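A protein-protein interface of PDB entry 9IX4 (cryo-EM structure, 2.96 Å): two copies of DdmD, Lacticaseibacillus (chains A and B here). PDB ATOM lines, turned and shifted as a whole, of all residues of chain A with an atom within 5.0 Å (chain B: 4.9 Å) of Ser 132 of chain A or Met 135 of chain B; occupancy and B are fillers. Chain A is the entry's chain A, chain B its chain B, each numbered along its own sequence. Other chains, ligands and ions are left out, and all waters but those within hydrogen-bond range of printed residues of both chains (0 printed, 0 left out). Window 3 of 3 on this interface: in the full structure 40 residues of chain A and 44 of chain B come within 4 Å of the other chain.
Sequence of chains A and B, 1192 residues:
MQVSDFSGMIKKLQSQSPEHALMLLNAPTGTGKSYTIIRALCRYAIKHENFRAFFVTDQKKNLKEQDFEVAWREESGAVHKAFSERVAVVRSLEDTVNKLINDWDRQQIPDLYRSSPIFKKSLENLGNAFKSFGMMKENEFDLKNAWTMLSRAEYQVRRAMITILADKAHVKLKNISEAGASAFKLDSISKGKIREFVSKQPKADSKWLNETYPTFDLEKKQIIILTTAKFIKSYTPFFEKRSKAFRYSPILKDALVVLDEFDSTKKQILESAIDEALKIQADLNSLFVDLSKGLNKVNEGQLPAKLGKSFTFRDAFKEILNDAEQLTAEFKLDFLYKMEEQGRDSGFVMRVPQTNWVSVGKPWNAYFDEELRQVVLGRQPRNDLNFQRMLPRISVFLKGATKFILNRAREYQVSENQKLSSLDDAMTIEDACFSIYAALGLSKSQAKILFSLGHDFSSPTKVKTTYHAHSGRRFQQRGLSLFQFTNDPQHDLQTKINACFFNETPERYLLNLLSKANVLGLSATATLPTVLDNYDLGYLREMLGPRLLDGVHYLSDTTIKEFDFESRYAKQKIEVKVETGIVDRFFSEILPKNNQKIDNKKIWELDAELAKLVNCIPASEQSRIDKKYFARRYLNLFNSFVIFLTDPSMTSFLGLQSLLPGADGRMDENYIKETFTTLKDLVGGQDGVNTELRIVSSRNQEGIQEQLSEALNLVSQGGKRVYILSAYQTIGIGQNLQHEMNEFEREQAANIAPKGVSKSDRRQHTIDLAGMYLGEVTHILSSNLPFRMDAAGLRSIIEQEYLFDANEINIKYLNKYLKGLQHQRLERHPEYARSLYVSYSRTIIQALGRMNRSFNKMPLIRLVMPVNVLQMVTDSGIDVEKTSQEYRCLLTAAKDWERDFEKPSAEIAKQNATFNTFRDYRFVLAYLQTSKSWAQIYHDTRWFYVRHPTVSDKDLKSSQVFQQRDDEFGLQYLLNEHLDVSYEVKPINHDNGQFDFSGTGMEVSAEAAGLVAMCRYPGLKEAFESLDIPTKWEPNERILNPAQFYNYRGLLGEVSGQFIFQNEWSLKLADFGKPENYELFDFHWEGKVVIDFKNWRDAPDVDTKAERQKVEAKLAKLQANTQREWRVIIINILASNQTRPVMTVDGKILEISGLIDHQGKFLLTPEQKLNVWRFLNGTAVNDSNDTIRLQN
OD1 of Asn 128 of chain A lies close to O of Met 135 of chain B (3.3 Å). OG of Ser 132 of chain A is in hydrogen-bond range of SD of Met 136 of chain B, 3.5 Å away.
The side-chain hydroxyl (OG) of Ser 132 of chain A lies within hydrogen-bond range of the backbone carbonyl oxygen (O) of Ala 129 of chain A.
Among the printed residues, pairs that only touch across the chains: Asn 128 of chain A with Met 136 of chain B (3.9 Å), Ser 132 of chain A with Ser 132 of chain B (3.9 Å), Ser 132 of chain A with Met 135 of chain B (3.9 Å), Met 135 of chain A with Lys 131 of chain B (3.6 Å) and Met 135 of chain A with Met 135 of chain B (3.6 Å).
Printed residues of chain B within 4 Å of Ser 132 of chain A: Ser 132, Met 135 and Met 136. Met 135 of chain B touches just these residues of chain A: Asn 128 (3.3 Å), Ser 132 (3.9 Å) and Met 135 (3.6 Å). Of the printed residues of chain A, Met 136 of chain B touches Asn 128 (3.9 Å) and Ser 132 (3.5 Å). Of the printed residues of chain A, Lys 131 of chain B touches Met 135 (3.6 Å). Of the printed residues of chain B, Met 135 of chain A touches Lys 131 (3.6 Å) and Met 135 (3.6 Å). Gly 134 of chain A touches none of the printed residues of chain B. The nearest printed residue of chain B that does not touch Ser 132 of chain A is Lys 131 of chain B (6.5 Å).
Of the 8 printed residues of chain B, 4 touch a printed residue of chain A. Printed residues of chain B that touch a printed residue of chain A: Lys 131, Ser 132, Met 135 and Met 136. Of the 9 printed residues of chain A, 3 touch a printed residue of chain B. Among the printed residues, 7 pairs touch across the chains.
Ser 132 of chain A touches Met 135 of chain B, but with the chains exchanged Met 135 of chain A does not touch Ser 132 of chain B (4.3 Å). Ser 132 of chain A touches Met 136 of chain B, but with the chains exchanged Met 136 of chain A does not touch Ser 132 of chain B (4.03 Å). Met 135 of chain A touches Lys 131 of chain B, but with the chains exchanged Lys 131 of chain A does not touch Met 135 of chain B (4.8 Å). Met 135 of chain A touches its own counterpart, Met 135 of chain B. 6 positions are printed for both chains.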
ATOM      1  N   ASN A 128      -1.032  24.831  32.864  1.00  0.00           N
ATOM      2  CA  ASN A 128      -0.905  25.186  31.455  1.00  0.00           C
ATOM      3  C   ASN A 128      -0.078  26.455  31.280  1.00  0.00           C
ATOM      4  O   ASN A 128       0.799  26.527  30.405  1.00  0.00           O
ATOM      5  CB  ASN A 128      -2.291  25.360  30.839  1.00  0.00           C
ATOM      6  CG  ASN A 128      -2.233  25.734  29.379  1.00  0.00           C
ATOM      7  OD1 ASN A 128      -2.699  26.800  28.981  1.00  0.00           O
ATOM      8  ND2 ASN A 128      -1.663  24.852  28.567  1.00  0.00           N
ATOM      9  N   ALA A 129      -0.338  27.464  32.114  1.00  0.00           N
ATOM     10  CA  ALA A 129       0.417  28.706  32.039  1.00  0.00           C
ATOM     11  C   ALA A 129       1.889  28.474  32.341  1.00  0.00           C
ATOM     12  O   ALA A 129       2.760  29.061  31.696  1.00  0.00           O
ATOM     13  CB  ALA A 129      -0.169  29.737  33.000  1.00  0.00           C
ATOM     14  N   PHE A 130       2.184  27.626  33.325  1.00  0.00           N
ATOM     15  CA  PHE A 130       3.571  27.339  33.661  1.00  0.00           C
ATOM     16  C   PHE A 130       4.260  26.577  32.541  1.00  0.00           C
ATOM     17  O   PHE A 130       5.445  26.800  32.269  1.00  0.00           O
ATOM     18  CB  PHE A 130       3.648  26.556  34.966  1.00  0.00           C
ATOM     19  CG  PHE A 130       5.047  26.278  35.415  1.00  0.00           C
ATOM     20  CD1 PHE A 130       5.922  27.314  35.675  1.00  0.00           C
ATOM     21  CD2 PHE A 130       5.490  24.981  35.569  1.00  0.00           C
ATOM     22  CE1 PHE A 130       7.210  27.061  36.083  1.00  0.00           C
ATOM     23  CE2 PHE A 130       6.776  24.721  35.977  1.00  0.00           C
ATOM     24  CZ  PHE A 130       7.638  25.763  36.235  1.00  0.00           C
ATOM     25  N   LYS A 131       3.539  25.667  31.885  1.00  0.00           N
ATOM     26  CA  LYS A 131       4.103  24.975  30.732  1.00  0.00           C
ATOM     27  C   LYS A 131       4.457  25.963  29.632  1.00  0.00           C
ATOM     28  O   LYS A 131       5.550  25.906  29.055  1.00  0.00           O
ATOM     29  CB  LYS A 131       3.119  23.925  30.222  1.00  0.00           C
ATOM     30  CG  LYS A 131       3.050  22.678  31.082  1.00  0.00           C
ATOM     31  CD  LYS A 131       2.011  21.702  30.558  1.00  0.00           C
ATOM     32  CE  LYS A 131       2.178  21.468  29.066  1.00  0.00           C
ATOM     33  NZ  LYS A 131       3.548  21.003  28.718  1.00  0.00           N
ATOM     34  N   SER A 132       3.548  26.896  29.341  1.00  0.00           N
ATOM     35  CA  SER A 132       3.837  27.903  28.323  1.00  0.00           C
ATOM     36  C   SER A 132       5.008  28.785  28.737  1.00  0.00           C
ATOM     37  O   SER A 132       5.868  29.119  27.913  1.00  0.00           O
ATOM     38  CB  SER A 132       2.599  28.754  28.056  1.00  0.00           C
ATOM     39  OG  SER A 132       2.334  29.609  29.149  1.00  0.00           O
ATOM     40  N   PHE A 133       5.053  29.172  30.013  1.00  0.00           N
ATOM     41  CA  PHE A 133       6.118  30.037  30.508  1.00  0.00           C
ATOM     42  C   PHE A 133       7.475  29.360  30.387  1.00  0.00           C
ATOM     43  O   PHE A 133       8.446  29.974  29.930  1.00  0.00           O
ATOM     44  CB  PHE A 133       5.818  30.424  31.958  1.00  0.00           C
ATOM     45  CG  PHE A 133       7.003  30.946  32.716  1.00  0.00           C
ATOM     46  CD1 PHE A 133       7.518  32.198  32.446  1.00  0.00           C
ATOM     47  CD2 PHE A 133       7.585  30.192  33.716  1.00  0.00           C
ATOM     48  CE1 PHE A 133       8.600  32.682  33.148  1.00  0.00           C
ATOM     49  CE2 PHE A 133       8.668  30.672  34.420  1.00  0.00           C
ATOM     50  CZ  PHE A 133       9.174  31.919  34.134  1.00  0.00           C
ATOM     51  N   GLY A 134       7.557  28.088  30.775  1.00  0.00           N
ATOM     52  CA  GLY A 134       8.792  27.349  30.585  1.00  0.00           C
ATOM     53  C   GLY A 134       9.140  27.191  29.119  1.00  0.00           C
ATOM     54  O   GLY A 134      10.317  27.190  28.747  1.00  0.00           O
ATOM     55  N   MET A 135       8.123  27.056  28.267  1.00  0.00           N
ATOM     56  CA  MET A 135       8.370  26.975  26.834  1.00  0.00           C
ATOM     57  C   MET A 135       8.981  28.263  26.299  1.00  0.00           C
ATOM     58  O   MET A 135       9.665  28.243  25.271  1.00  0.00           O
ATOM     59  CB  MET A 135       7.067  26.657  26.103  1.00  0.00           C
ATOM     60  CG  MET A 135       7.229  26.354  24.628  1.00  0.00           C
ATOM     61  SD  MET A 135       5.681  25.845  23.865  1.00  0.00           S
ATOM     62  CE  MET A 135       5.503  24.199  24.542  1.00  0.00           C
ATOM     63  N   MET A 136       8.765  29.382  26.986  1.00  0.00           N
ATOM     64  CA  MET A 136       9.222  30.693  26.531  1.00  0.00           C
ATOM     65  C   MET A 136      10.266  31.286  27.470  1.00  0.00           C
ATOM     66  O   MET A 136      10.216  32.470  27.811  1.00  0.00           O
ATOM     67  CB  MET A 136       8.032  31.634  26.375  1.00  0.00           C
ATOM     68  CG  MET A 136       8.289  32.823  25.471  1.00  0.00           C
ATOM     69  SD  MET A 136       8.846  32.316  23.837  1.00  0.00           S
ATOM     70  CE  MET A 136       7.352  31.570  23.203  1.00  0.00           C
ATOM     71  N   LYS B 131       3.037  27.890  19.218  1.00  0.00           N
ATOM     72  CA  LYS B 131       2.534  26.890  20.151  1.00  0.00           C
ATOM     73  C   LYS B 131       2.088  27.538  21.454  1.00  0.00           C
ATOM     74  O   LYS B 131       1.021  27.211  21.990  1.00  0.00           O
ATOM     75  CB  LYS B 131       3.606  25.837  20.418  1.00  0.00           C
ATOM     76  CG  LYS B 131       3.632  24.719  19.400  1.00  0.00           C
ATOM     77  CD  LYS B 131       4.579  23.605  19.816  1.00  0.00           C
ATOM     78  CE  LYS B 131       4.338  23.169  21.251  1.00  0.00           C
ATOM     79  NZ  LYS B 131       2.932  22.743  21.489  1.00  0.00           N
ATOM     80  N   SER B 132       2.888  28.471  21.971  1.00  0.00           N
ATOM     81  CA  SER B 132       2.505  29.169  23.195  1.00  0.00           C
ATOM     82  C   SER B 132       1.232  29.984  22.995  1.00  0.00           C
ATOM     83  O   SER B 132       0.363  30.025  23.876  1.00  0.00           O
ATOM     84  CB  SER B 132       3.646  30.066  23.663  1.00  0.00           C
ATOM     85  OG  SER B 132       3.272  30.795  24.815  1.00  0.00           O
ATOM     86  N   PHE B 133       1.117  30.653  21.848  1.00  0.00           N
ATOM     87  CA  PHE B 133      -0.067  31.451  21.554  1.00  0.00           C
ATOM     88  C   PHE B 133      -1.307  30.576  21.474  1.00  0.00           C
ATOM     89  O   PHE B 133      -2.383  30.962  21.941  1.00  0.00           O
ATOM     90  CB  PHE B 133       0.144  32.217  20.250  1.00  0.00           C
ATOM     91  CG  PHE B 133      -1.050  33.003  19.800  1.00  0.00           C
ATOM     92  CD1 PHE B 133      -1.344  34.225  20.374  1.00  0.00           C
ATOM     93  CD2 PHE B 133      -1.865  32.532  18.791  1.00  0.00           C
ATOM     94  CE1 PHE B 133      -2.434  34.954  19.958  1.00  0.00           C
ATOM     95  CE2 PHE B 133      -2.957  33.256  18.373  1.00  0.00           C
ATOM     96  CZ  PHE B 133      -3.241  34.468  18.956  1.00  0.00           C
ATOM     97  N   GLY B 134      -1.177  29.394  20.874  1.00  0.00           N
ATOM     98  CA  GLY B 134      -2.289  28.461  20.856  1.00  0.00           C
ATOM     99  C   GLY B 134      -2.659  27.975  22.243  1.00  0.00           C
ATOM    100  O   GLY B 134      -3.841  27.821  22.561  1.00  0.00           O
ATOM    101  N   MET B 135      -1.657  27.724  23.086  1.00  0.00           N
ATOM    102  CA  MET B 135      -1.947  27.275  24.444  1.00  0.00           C
ATOM    103  C   MET B 135      -2.666  28.352  25.246  1.00  0.00           C
ATOM    104  O   MET B 135      -3.581  28.048  26.020  1.00  0.00           O
ATOM    105  CB  MET B 135      -0.663  26.853  25.156  1.00  0.00           C
ATOM    106  CG  MET B 135      -0.318  25.387  24.984  1.00  0.00           C
ATOM    107  SD  MET B 135       1.182  24.910  25.858  1.00  0.00           S
ATOM    108  CE  MET B 135       2.352  26.079  25.183  1.00  0.00           C
ATOM    109  N   MET B 136      -2.273  29.613  25.075  1.00  0.00           N
ATOM    110  CA  MET B 136      -2.807  30.704  25.879  1.00  0.00           C
ATOM    111  C   MET B 136      -4.046  31.346  25.266  1.00  0.00           C
ATOM    112  O   MET B 136      -4.322  32.517  25.540  1.00  0.00           O
ATOM    113  CB  MET B 136      -1.734  31.771  26.102  1.00  0.00           C
ATOM    114  CG  MET B 136      -0.537  31.294  26.900  1.00  0.00           C
ATOM    115  SD  MET B 136      -0.979  30.178  28.245  1.00  0.00           S
ATOM    116  CE  MET B 136      -1.743  31.310  29.401  1.00  0.00           C
ATOM    117  N   LYS B 137      -4.803  30.608  24.456  1.00  0.00           N
ATOM    118  CA  LYS B 137      -5.968  31.175  23.790  1.00  0.00           C
ATOM    119  C   LYS B 137      -7.212  31.200  24.666  1.00  0.00           C
ATOM    120  O   LYS B 137      -8.233  31.749  24.240  1.00  0.00           O
ATOM    121  CB  LYS B 137      -6.267  30.400  22.504  1.00  0.00           C
ATOM    122  CG  LYS B 137      -5.549  30.935  21.281  1.00  0.00           C
ATOM    123  CD  LYS B 137      -5.623  29.953  20.125  1.00  0.00           C
ATOM    124  CE  LYS B 137      -6.990  29.971  19.466  1.00  0.00           C
ATOM    125  NZ  LYS B 137      -7.350  31.324  18.964  1.00  0.00           N
ATOM    126  N   GLU B 138      -7.157  30.631  25.870  1.00  0.00           N
ATOM    127  CA  GLU B 138      -8.353  30.551  26.704  1.00  0.00           C
ATOM    128  C   GLU B 138      -8.719  31.912  27.282  1.00  0.00           C
ATOM    129  O   GLU B 138      -9.800  32.445  27.013  1.00  0.00           O
ATOM    130  CB  GLU B 138      -8.142  29.527  27.820  1.00  0.00           C
ATOM    131  CG  GLU B 138      -8.619  28.130  27.468  1.00  0.00           C
ATOM    132  CD  GLU B 138      -7.787  27.492  26.374  1.00  0.00           C
ATOM    133  OE1 GLU B 138      -6.591  27.828  26.262  1.00  0.00           O
ATOM    134  OE2 GLU B 138      -8.330  26.656  25.623  1.00  0.00           O
